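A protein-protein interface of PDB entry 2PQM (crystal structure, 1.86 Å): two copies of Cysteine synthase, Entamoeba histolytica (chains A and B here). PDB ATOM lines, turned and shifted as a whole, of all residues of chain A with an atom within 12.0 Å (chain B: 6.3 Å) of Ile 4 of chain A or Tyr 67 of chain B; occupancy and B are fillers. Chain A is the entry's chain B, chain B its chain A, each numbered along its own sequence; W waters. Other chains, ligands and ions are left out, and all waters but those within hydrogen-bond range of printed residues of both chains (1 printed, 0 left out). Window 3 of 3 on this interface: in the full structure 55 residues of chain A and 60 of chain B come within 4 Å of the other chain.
Printed residues of chain B that touch a printed residue of chain A: Arg 12, Asn 16, Leu 18, Glu 19, Phe 63, Tyr 67 and Val 99. Hydrophobic or aromatic side chains of chain B within 4 Å of the printed part of chain A: Leu 18, Phe 63, Tyr 67 and Val 99. Of the 12 printed residues of chain A, 6 touch a printed residue of chain B. Printed residues of chain A that touch a printed residue of chain B: Ile 4, Ser 5, Ile 6, Ser 7, Val 27 and Asp 273. Hydrophobic or aromatic side chains of chain A within 4 Å of the printed part of chain B: Ile 4, Ile 6 and Val 27. Among the printed residues, no Asp or Glu carboxylate lies within 4 Å of a Lys or Arg side-chain nitrogen of the other chain.
Printed residues of chain B within 4 Å of Ile 4 of chain A: Asn 16, Leu 18, Phe 63 and Tyr 67. Tyr 67 of chain B touches one residue of chain A. Glu 19 of chain B touches just these residues of chain A: Ser 5, Ile 6 and Ser 7. No residue of chain A comes within 4 Å of Gly 62 of chain B. Of chain A, only Ile 4 and Ile 6 come within 4 Å of Phe 63 of chain B. No residue of chain A comes within 4 Å of Asn 64 of chain B. No residue of chain A comes within 4 Å of Gln 68 of chain B. Of the printed residues of chain B, Asp 273 of chain A touches Val 99 (3.8 Å). Of the printed residues of chain A, Val 99 of chain B touches Asp 273 (3.8 Å). Printed residues of chain B within 4 Å of Ser 5 of chain A: Arg 12 and Glu 19. Of the printed residues of chain B, Ser 7 of chain A touches Glu 19. The nearest printed residue of chain B that does not touch Ile 4 of chain A is Glu 19 of chain B (4.1 Å).
No position is printed for both chains. Of the 13 pairs that touch across the chains among the printed residues, none has its exchanged pair printed and touching as well.
The guanidinium group of Arg 12 of chain B sits at hydrogen-bond distance from the backbone carbonyl oxygen of Ser 5 of chain A, 3.2 Å away. The backbone carbonyl oxygen (O) of Glu 19 of chain B lies within hydrogen-bond range of the side-chain hydroxyl (OG) of Ser 7 of chain A (2.8 Å).
Asn 16 of chain B touches Ile 4 of chain A (ND2 to CD1, 3.6 Å). CD1 of Ile 4 of chain A touches CD1 of Leu 18 of chain B (3.999 Å). Phe 63 of chain B touches Ile 4 of chain A. Ser 5 of chain A touches Glu 19 of chain B. Ile 6 of chain A touches Arg 12 of chain B. Leu 18 of chain B touches Ile 6 of chain A (O to CG2, 3.8 Å). Ile 6 of chain A touches Glu 19 of chain B (C to O, 3.7 Å). Ile 6 of chain A touches Phe 63 of chain B (CG2 to CE2, 3.6 Å). Val 27 of chain A touches Asn 16 of chain B. Asp 273 of chain A touches Val 99 of chain B.
The guanidinium group of Arg 12 of chain B is in salt-bridge range of the side-chain carboxylate of Glu 19 of chain B, at 3.1 Å. The side-chain amide oxygen (OD1) of Asn 16 of chain B is in hydrogen-bond range of the backbone NH (N) of Leu 18 of chain B (2.9 Å). The backbone NH of Glu 19 of chain B is in hydrogen-bond range of the side-chain amide oxygen of Asn 16 of chain B, 3.4 Å away. The backbone NH (N) of His 30 of chain A lies within hydrogen-bond range of the side-chain carboxylate (OD1) of Asp 273 of chain A, 2.8 Å away.
Water W1 bridges N of Ser 8 of chain A and NH1 of Arg 12 of chain B.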
ATOM      1  N   GLN A   3      -9.118 -19.554  12.671  1.00  0.00           N
ATOM      2  CA  GLN A   3     -10.613 -19.555  12.779  1.00  0.00           C
ATOM      3  C   GLN A   3     -11.201 -18.363  12.022  1.00  0.00           C
ATOM      4  O   GLN A   3     -10.607 -17.277  11.957  1.00  0.00           O
ATOM      5  CB  GLN A   3     -11.051 -19.545  14.228  1.00  0.00           C
ATOM      6  N   ILE A   4     -12.370 -18.579  11.435  1.00  0.00           N
ATOM      7  CA  ILE A   4     -12.959 -17.602  10.529  1.00  0.00           C
ATOM      8  C   ILE A   4     -14.462 -17.495  10.833  1.00  0.00           C
ATOM      9  O   ILE A   4     -15.223 -18.442  10.603  1.00  0.00           O
ATOM     10  CB  ILE A   4     -12.663 -18.023   9.066  1.00  0.00           C
ATOM     11  CG1 ILE A   4     -12.712 -16.857   8.092  1.00  0.00           C
ATOM     12  CG2 ILE A   4     -13.585 -19.105   8.615  1.00  0.00           C
ATOM     13  CD1 ILE A   4     -11.850 -17.131   6.871  1.00  0.00           C
ATOM     14  N   SER A   5     -14.883 -16.357  11.380  1.00  0.00           N
ATOM     15  CA  SER A   5     -16.285 -16.179  11.754  1.00  0.00           C
ATOM     16  C   SER A   5     -16.940 -15.269  10.735  1.00  0.00           C
ATOM     17  O   SER A   5     -16.409 -14.196  10.417  1.00  0.00           O
ATOM     18  CB  SER A   5     -16.428 -15.548  13.145  1.00  0.00           C
ATOM     19  OG  SER A   5     -15.358 -15.919  13.988  1.00  0.00           O
ATOM     20  N   ILE A   6     -18.094 -15.687  10.237  1.00  0.00           N
ATOM     21  CA  ILE A   6     -18.901 -14.805   9.369  1.00  0.00           C
ATOM     22  C   ILE A   6     -19.646 -13.759  10.187  1.00  0.00           C
ATOM     23  O   ILE A   6     -19.503 -13.728  11.422  1.00  0.00           O
ATOM     24  CB  ILE A   6     -19.850 -15.596   8.444  1.00  0.00           C
ATOM     25  CG1 ILE A   6     -20.908 -16.375   9.241  1.00  0.00           C
ATOM     26  CG2 ILE A   6     -19.032 -16.468   7.478  1.00  0.00           C
ATOM     27  CD1 ILE A   6     -22.087 -16.871   8.345  1.00  0.00           C
ATOM     28  N   SER A   7     -20.406 -12.881   9.526  1.00  0.00           N
ATOM     29  CA  SER A   7     -21.045 -11.760  10.241  1.00  0.00           C
ATOM     30  C   SER A   7     -22.229 -12.195  11.090  1.00  0.00           C
ATOM     31  O   SER A   7     -22.949 -13.145  10.757  1.00  0.00           O
ATOM     32  CB  SER A   7     -21.456 -10.630   9.297  1.00  0.00           C
ATOM     33  OG  SER A   7     -20.308 -10.099   8.649  1.00  0.00           O
ATOM     34  N   SER A   8     -22.423 -11.486  12.196  1.00  0.00           N
ATOM     35  CA  SER A   8     -23.513 -11.763  13.122  1.00  0.00           C
ATOM     36  C   SER A   8     -24.768 -11.026  12.643  1.00  0.00           C
ATOM     37  O   SER A   8     -24.670 -10.123  11.790  1.00  0.00           O
ATOM     38  CB  SER A   8     -23.138 -11.264  14.529  1.00  0.00           C
ATOM     39  OG  SER A   8     -22.082 -12.065  15.042  1.00  0.00           O
ATOM     40  N   VAL A  27     -12.031  -3.811   5.923  1.00  0.00           N
ATOM     41  CA  VAL A  27     -11.465  -5.163   5.747  1.00  0.00           C
ATOM     42  C   VAL A  27      -9.952  -5.069   5.556  1.00  0.00           C
ATOM     43  O   VAL A  27      -9.466  -4.250   4.745  1.00  0.00           O
ATOM     44  CB  VAL A  27     -12.089  -5.864   4.510  1.00  0.00           C
ATOM     45  CG1 VAL A  27     -11.498  -7.273   4.309  1.00  0.00           C
ATOM     46  CG2 VAL A  27     -13.663  -5.850   4.586  1.00  0.00           C
ATOM     47  N   GLU A  28      -9.205  -5.893   6.298  1.00  0.00           N
ATOM     48  CA  GLU A  28      -7.733  -5.950   6.141  1.00  0.00           C
ATOM     49  C   GLU A  28      -7.289  -6.515   4.801  1.00  0.00           C
ATOM     50  O   GLU A  28      -7.843  -7.511   4.303  1.00  0.00           O
ATOM     51  CB  GLU A  28      -7.062  -6.806   7.230  1.00  0.00           C
ATOM     52  CG  GLU A  28      -7.408  -6.480   8.647  1.00  0.00           C
ATOM     53  CD  GLU A  28      -6.810  -7.485   9.654  1.00  0.00           C
ATOM     54  OE1 GLU A  28      -6.774  -8.711   9.399  1.00  0.00           O
ATOM     55  OE2 GLU A  28      -6.402  -7.036  10.744  1.00  0.00           O
ATOM     56  N   HIS A  30      -4.250  -8.409   2.816  1.00  0.00           N
ATOM     57  CA  HIS A  30      -3.174  -9.330   3.189  1.00  0.00           C
ATOM     58  C   HIS A  30      -2.367  -9.807   1.990  1.00  0.00           C
ATOM     59  O   HIS A  30      -1.118  -9.867   2.047  1.00  0.00           O
ATOM     60  CB  HIS A  30      -3.756 -10.537   3.940  1.00  0.00           C
ATOM     61  CG  HIS A  30      -4.283 -10.201   5.298  1.00  0.00           C
ATOM     62  ND1 HIS A  30      -3.470  -9.857   6.360  1.00  0.00           N
ATOM     63  CD2 HIS A  30      -5.551 -10.162   5.767  1.00  0.00           C
ATOM     64  CE1 HIS A  30      -4.216  -9.603   7.417  1.00  0.00           C
ATOM     65  NE2 HIS A  30      -5.484  -9.793   7.086  1.00  0.00           N
ATOM     66  N   ASP A 273      -6.464 -10.962  -2.890  1.00  0.00           N
ATOM     67  CA  ASP A 273      -7.301 -10.794  -1.698  1.00  0.00           C
ATOM     68  C   ASP A 273      -8.756 -11.224  -1.869  1.00  0.00           C
ATOM     69  O   ASP A 273      -9.505 -11.231  -0.901  1.00  0.00           O
ATOM     70  CB  ASP A 273      -7.225  -9.357  -1.177  1.00  0.00           C
ATOM     71  CG  ASP A 273      -5.931  -9.090  -0.448  1.00  0.00           C
ATOM     72  OD1 ASP A 273      -5.831  -9.420   0.768  1.00  0.00           O
ATOM     73  OD2 ASP A 273      -5.005  -8.571  -1.103  1.00  0.00           O
ATOM     74  N   GLY A 274      -9.162 -11.574  -3.089  1.00  0.00           N
ATOM     75  CA  GLY A 274     -10.556 -12.010  -3.291  1.00  0.00           C
ATOM     76  C   GLY A 274     -11.559 -10.885  -3.144  1.00  0.00           C
ATOM     77  O   GLY A 274     -12.735 -11.127  -2.879  1.00  0.00           O
ATOM     78  N   ILE A 275     -11.091  -9.652  -3.347  1.00  0.00           N
ATOM     79  CA  ILE A 275     -11.898  -8.441  -3.208  1.00  0.00           C
ATOM     80  C   ILE A 275     -12.034  -7.821  -4.593  1.00  0.00           C
ATOM     81  O   ILE A 275     -11.038  -7.373  -5.178  1.00  0.00           O
ATOM     82  CB  ILE A 275     -11.260  -7.454  -2.185  1.00  0.00           C
ATOM     83  CG1 ILE A 275     -11.398  -8.014  -0.751  1.00  0.00           C
ATOM     84  CG2 ILE A 275     -11.943  -6.063  -2.267  1.00  0.00           C
ATOM     85  CD1 ILE A 275     -10.514  -7.287   0.291  1.00  0.00           C
ATOM     86  N   ARG B  12     -16.183  -3.232  13.783  1.00  0.00           N
ATOM     87  CA  ARG B  12     -15.431  -4.473  13.538  1.00  0.00           C
ATOM     88  C   ARG B  12     -14.437  -4.147  12.428  1.00  0.00           C
ATOM     89  O   ARG B  12     -14.736  -3.326  11.536  1.00  0.00           O
ATOM     90  CB  ARG B  12     -16.357  -5.659  13.114  1.00  0.00           C
ATOM     91  CG  ARG B  12     -15.627  -7.042  13.028  1.00  0.00           C
ATOM     92  CD  ARG B  12     -16.506  -8.292  12.808  1.00  0.00           C
ATOM     93  NE  ARG B  12     -15.665  -9.484  12.554  1.00  0.00           N
ATOM     94  CZ  ARG B  12     -16.088 -10.647  12.069  1.00  0.00           C
ATOM     95  NH1 ARG B  12     -17.372 -10.859  11.740  1.00  0.00           N
ATOM     96  NH2 ARG B  12     -15.211 -11.633  11.913  1.00  0.00           N
ATOM     97  N   ASN B  16     -10.622 -10.615   6.588  1.00  0.00           N
ATOM     98  CA  ASN B  16     -10.678 -10.836   5.162  1.00  0.00           C
ATOM     99  C   ASN B  16     -12.142 -10.762   4.722  1.00  0.00           C
ATOM    100  O   ASN B  16     -13.054 -10.650   5.560  1.00  0.00           O
ATOM    101  CB  ASN B  16     -10.079 -12.209   4.779  1.00  0.00           C
ATOM    102  CG  ASN B  16     -10.770 -13.347   5.490  1.00  0.00           C
ATOM    103  OD1 ASN B  16     -11.986 -13.538   5.347  1.00  0.00           O
ATOM    104  ND2 ASN B  16     -10.018 -14.090   6.314  1.00  0.00           N
ATOM    105  N   LEU B  18     -14.205 -12.878   3.569  1.00  0.00           N
ATOM    106  CA  LEU B  18     -15.137 -13.936   3.933  1.00  0.00           C
ATOM    107  C   LEU B  18     -15.844 -13.619   5.230  1.00  0.00           C
ATOM    108  O   LEU B  18     -16.937 -14.070   5.428  1.00  0.00           O
ATOM    109  CB  LEU B  18     -14.424 -15.309   4.032  1.00  0.00           C
ATOM    110  CG  LEU B  18     -13.664 -15.733   2.774  1.00  0.00           C
ATOM    111  CD1 LEU B  18     -12.970 -17.122   3.032  1.00  0.00           C
ATOM    112  CD2 LEU B  18     -14.531 -15.761   1.472  1.00  0.00           C
ATOM    113  N   GLU B  19     -15.225 -12.816   6.103  1.00  0.00           N
ATOM    114  CA  GLU B  19     -15.860 -12.479   7.365  1.00  0.00           C
ATOM    115  C   GLU B  19     -17.014 -11.526   7.204  1.00  0.00           C
ATOM    116  O   GLU B  19     -17.780 -11.307   8.160  1.00  0.00           O
ATOM    117  CB  GLU B  19     -14.839 -11.905   8.332  1.00  0.00           C
ATOM    118  CG  GLU B  19     -13.830 -12.995   8.798  1.00  0.00           C
ATOM    119  CD  GLU B  19     -12.924 -12.553   9.948  1.00  0.00           C
ATOM    120  OE1 GLU B  19     -12.707 -11.359  10.139  1.00  0.00           O
ATOM    121  OE2 GLU B  19     -12.388 -13.433  10.648  1.00  0.00           O
ATOM    122  N   GLY B  62     -20.569 -21.211  -1.046  1.00  0.00           N
ATOM    123  CA  GLY B  62     -19.172 -21.339  -1.468  1.00  0.00           C
ATOM    124  C   GLY B  62     -18.248 -21.304  -0.256  1.00  0.00           C
ATOM    125  O   GLY B  62     -17.360 -22.149  -0.117  1.00  0.00           O
ATOM    126  N   PHE B  63     -18.506 -20.379   0.661  1.00  0.00           N
ATOM    127  CA  PHE B  63     -17.688 -20.295   1.863  1.00  0.00           C
ATOM    128  C   PHE B  63     -17.799 -21.545   2.720  1.00  0.00           C
ATOM    129  O   PHE B  63     -16.779 -22.129   3.089  1.00  0.00           O
ATOM    130  CB  PHE B  63     -18.029 -19.083   2.736  1.00  0.00           C
ATOM    131  CG  PHE B  63     -17.353 -19.123   4.069  1.00  0.00           C
ATOM    132  CD1 PHE B  63     -15.978 -18.917   4.162  1.00  0.00           C
ATOM    133  CD2 PHE B  63     -18.066 -19.408   5.215  1.00  0.00           C
ATOM    134  CE1 PHE B  63     -15.334 -18.985   5.388  1.00  0.00           C
ATOM    135  CE2 PHE B  63     -17.426 -19.471   6.447  1.00  0.00           C
ATOM    136  CZ  PHE B  63     -16.056 -19.250   6.521  1.00  0.00           C
ATOM    137  N   ASN B  64     -19.015 -21.931   3.082  1.00  0.00           N
ATOM    138  CA  ASN B  64     -19.139 -23.041   4.041  1.00  0.00           C
ATOM    139  C   ASN B  64     -18.684 -24.382   3.462  1.00  0.00           C
ATOM    140  O   ASN B  64     -18.113 -25.219   4.178  1.00  0.00           O
ATOM    141  CB  ASN B  64     -20.549 -23.196   4.597  1.00  0.00           C
ATOM    142  CG  ASN B  64     -20.542 -23.915   5.935  1.00  0.00           C
ATOM    143  OD1 ASN B  64     -19.723 -23.590   6.791  1.00  0.00           O
ATOM    144  ND2 ASN B  64     -21.397 -24.931   6.099  1.00  0.00           N
ATOM    145  N   ILE B  65     -18.946 -24.581   2.172  1.00  0.00           N
ATOM    146  CA  ILE B  65     -18.479 -25.804   1.488  1.00  0.00           C
ATOM    147  C   ILE B  65     -16.946 -25.915   1.568  1.00  0.00           C
ATOM    148  O   ILE B  65     -16.402 -26.976   1.943  1.00  0.00           O
ATOM    149  CB  ILE B  65     -18.983 -25.867   0.019  1.00  0.00           C
ATOM    150  CG1 ILE B  65     -20.507 -26.164   0.028  1.00  0.00           C
ATOM    151  CG2 ILE B  65     -18.170 -26.925  -0.787  1.00  0.00           C
ATOM    152  CD1 ILE B  65     -21.173 -26.242  -1.390  1.00  0.00           C
ATOM    153  N   VAL B  66     -16.261 -24.829   1.223  1.00  0.00           N
ATOM    154  CA  VAL B  66     -14.782 -24.825   1.223  1.00  0.00           C
ATOM    155  C   VAL B  66     -14.222 -24.885   2.662  1.00  0.00           C
ATOM    156  O   VAL B  66     -13.329 -25.704   2.985  1.00  0.00           O
ATOM    157  CB  VAL B  66     -14.229 -23.654   0.358  1.00  0.00           C
ATOM    158  CG1 VAL B  66     -12.729 -23.491   0.517  1.00  0.00           C
ATOM    159  CG2 VAL B  66     -14.562 -23.902  -1.151  1.00  0.00           C
ATOM    160  N   TYR B  67     -14.759 -24.051   3.542  1.00  0.00           N
ATOM    161  CA  TYR B  67     -14.313 -24.027   4.939  1.00  0.00           C
ATOM    162  C   TYR B  67     -14.514 -25.358   5.679  1.00  0.00           C
ATOM    163  O   TYR B  67     -13.611 -25.844   6.376  1.00  0.00           O
ATOM    164  CB  TYR B  67     -15.055 -22.915   5.654  1.00  0.00           C
ATOM    165  CG  TYR B  67     -14.674 -22.664   7.071  1.00  0.00           C
ATOM    166  CD1 TYR B  67     -13.369 -22.311   7.417  1.00  0.00           C
ATOM    167  CD2 TYR B  67     -15.651 -22.688   8.068  1.00  0.00           C
ATOM    168  CE1 TYR B  67     -13.030 -22.061   8.750  1.00  0.00           C
ATOM    169  CE2 TYR B  67     -15.328 -22.425   9.398  1.00  0.00           C
ATOM    170  CZ  TYR B  67     -14.025 -22.104   9.727  1.00  0.00           C
ATOM    171  OH  TYR B  67     -13.725 -21.844  11.051  1.00  0.00           O
ATOM    172  N   GLN B  68     -15.697 -25.941   5.550  1.00  0.00           N
ATOM    173  CA  GLN B  68     -15.971 -27.194   6.228  1.00  0.00           C
ATOM    174  C   GLN B  68     -15.088 -28.321   5.653  1.00  0.00           C
ATOM    175  O   GLN B  68     -14.613 -29.196   6.409  1.00  0.00           O
ATOM    176  CB  GLN B  68     -17.455 -27.556   6.165  1.00  0.00           C
ATOM    177  CG  GLN B  68     -18.400 -26.581   6.861  1.00  0.00           C
ATOM    178  CD  GLN B  68     -18.114 -26.398   8.344  1.00  0.00           C
ATOM    179  OE1 GLN B  68     -17.754 -27.350   9.034  1.00  0.00           O
ATOM    180  NE2 GLN B  68     -18.310 -25.165   8.842  1.00  0.00           N
ATOM    181  N   ALA B  69     -14.839 -28.280   4.340  1.00  0.00           N
ATOM    182  CA  ALA B  69     -13.953 -29.272   3.702  1.00  0.00           C
ATOM    183  C   ALA B  69     -12.487 -29.137   4.203  1.00  0.00           C
ATOM    184  O   ALA B  69     -11.815 -30.145   4.469  1.00  0.00           O
ATOM    185  CB  ALA B  69     -14.005 -29.165   2.203  1.00  0.00           C
ATOM    186  N   ILE B  70     -12.006 -27.899   4.336  1.00  0.00           N
ATOM    187  CA  ILE B  70     -10.689 -27.668   4.925  1.00  0.00           C
ATOM    188  C   ILE B  70     -10.637 -28.176   6.373  1.00  0.00           C
ATOM    189  O   ILE B  70      -9.689 -28.870   6.745  1.00  0.00           O
ATOM    190  CB  ILE B  70     -10.218 -26.188   4.817  1.00  0.00           C
ATOM    191  CG1 ILE B  70     -10.008 -25.814   3.347  1.00  0.00           C
ATOM    192  CG2 ILE B  70      -8.917 -25.979   5.657  1.00  0.00           C
ATOM    193  CD1 ILE B  70      -9.846 -24.324   3.076  1.00  0.00           C
ATOM    194  N   LYS B  71     -11.668 -27.885   7.161  1.00  0.00           N
ATOM    195  CA  LYS B  71     -11.694 -28.286   8.564  1.00  0.00           C
ATOM    196  C   LYS B  71     -11.704 -29.802   8.757  1.00  0.00           C
ATOM    197  O   LYS B  71     -11.039 -30.307   9.687  1.00  0.00           O
ATOM    198  CB  LYS B  71     -12.874 -27.663   9.288  1.00  0.00           C
ATOM    199  CG  LYS B  71     -12.678 -26.177   9.638  1.00  0.00           C
ATOM    200  CD  LYS B  71     -13.966 -25.559  10.182  1.00  0.00           C
ATOM    201  CE  LYS B  71     -14.523 -26.308  11.368  1.00  0.00           C
ATOM    202  NZ  LYS B  71     -15.797 -25.659  11.846  1.00  0.00           N
ATOM    203  N   ASP B  72     -12.456 -30.488   7.881  1.00  0.00           N
ATOM    204  CA  ASP B  72     -12.627 -31.962   7.846  1.00  0.00           C
ATOM    205  C   ASP B  72     -11.468 -32.736   7.268  1.00  0.00           C
ATOM    206  O   ASP B  72     -11.361 -33.949   7.488  1.00  0.00           O
ATOM    207  CB  ASP B  72     -13.813 -32.315   6.929  1.00  0.00           C
ATOM    208  CG  ASP B  72     -15.130 -32.111   7.598  1.00  0.00           C
ATOM    209  OD1 ASP B  72     -15.132 -31.671   8.783  1.00  0.00           O
ATOM    210  OD2 ASP B  72     -16.169 -32.403   6.946  1.00  0.00           O
ATOM    211  N   ALA B  96     -14.054 -17.744  -2.203  1.00  0.00           N
ATOM    212  CA  ALA B  96     -13.509 -18.602  -1.127  1.00  0.00           C
ATOM    213  C   ALA B  96     -12.106 -19.133  -1.482  1.00  0.00           C
ATOM    214  O   ALA B  96     -11.172 -19.060  -0.668  1.00  0.00           O
ATOM    215  CB  ALA B  96     -14.471 -19.768  -0.830  1.00  0.00           C
ATOM    216  N   VAL B  99      -9.262 -16.517  -1.191  1.00  0.00           N
ATOM    217  CA  VAL B  99      -8.873 -16.182   0.182  1.00  0.00           C
ATOM    218  C   VAL B  99      -8.133 -17.351   0.834  1.00  0.00           C
ATOM    219  O   VAL B  99      -7.112 -17.143   1.475  1.00  0.00           O
ATOM    220  CB  VAL B  99     -10.103 -15.764   1.071  1.00  0.00           C
ATOM    221  CG1 VAL B  99      -9.690 -15.472   2.519  1.00  0.00           C
ATOM    222  CG2 VAL B  99     -10.779 -14.539   0.466  1.00  0.00           C
ATOM    223  N   PHE B 100      -8.662 -18.568   0.677  1.00  0.00           N
ATOM    224  CA  PHE B 100      -8.053 -19.761   1.287  1.00  0.00           C
ATOM    225  C   PHE B 100      -6.753 -20.192   0.579  1.00  0.00           C
ATOM    226  O   PHE B 100      -5.924 -20.907   1.163  1.00  0.00           O
ATOM    227  CB  PHE B 100      -9.060 -20.911   1.352  1.00  0.00           C
ATOM    228  CG  PHE B 100     -10.065 -20.791   2.474  1.00  0.00           C
ATOM    229  CD1 PHE B 100      -9.657 -20.785   3.811  1.00  0.00           C
ATOM    230  CD2 PHE B 100     -11.431 -20.703   2.193  1.00  0.00           C
ATOM    231  CE1 PHE B 100     -10.604 -20.679   4.849  1.00  0.00           C
ATOM    232  CE2 PHE B 100     -12.367 -20.609   3.218  1.00  0.00           C
ATOM    233  CZ  PHE B 100     -11.962 -20.588   4.540  1.00  0.00           C
HETATM  234  O   HOH W   1     -20.114  -9.646  13.117  1.00  0.00           O
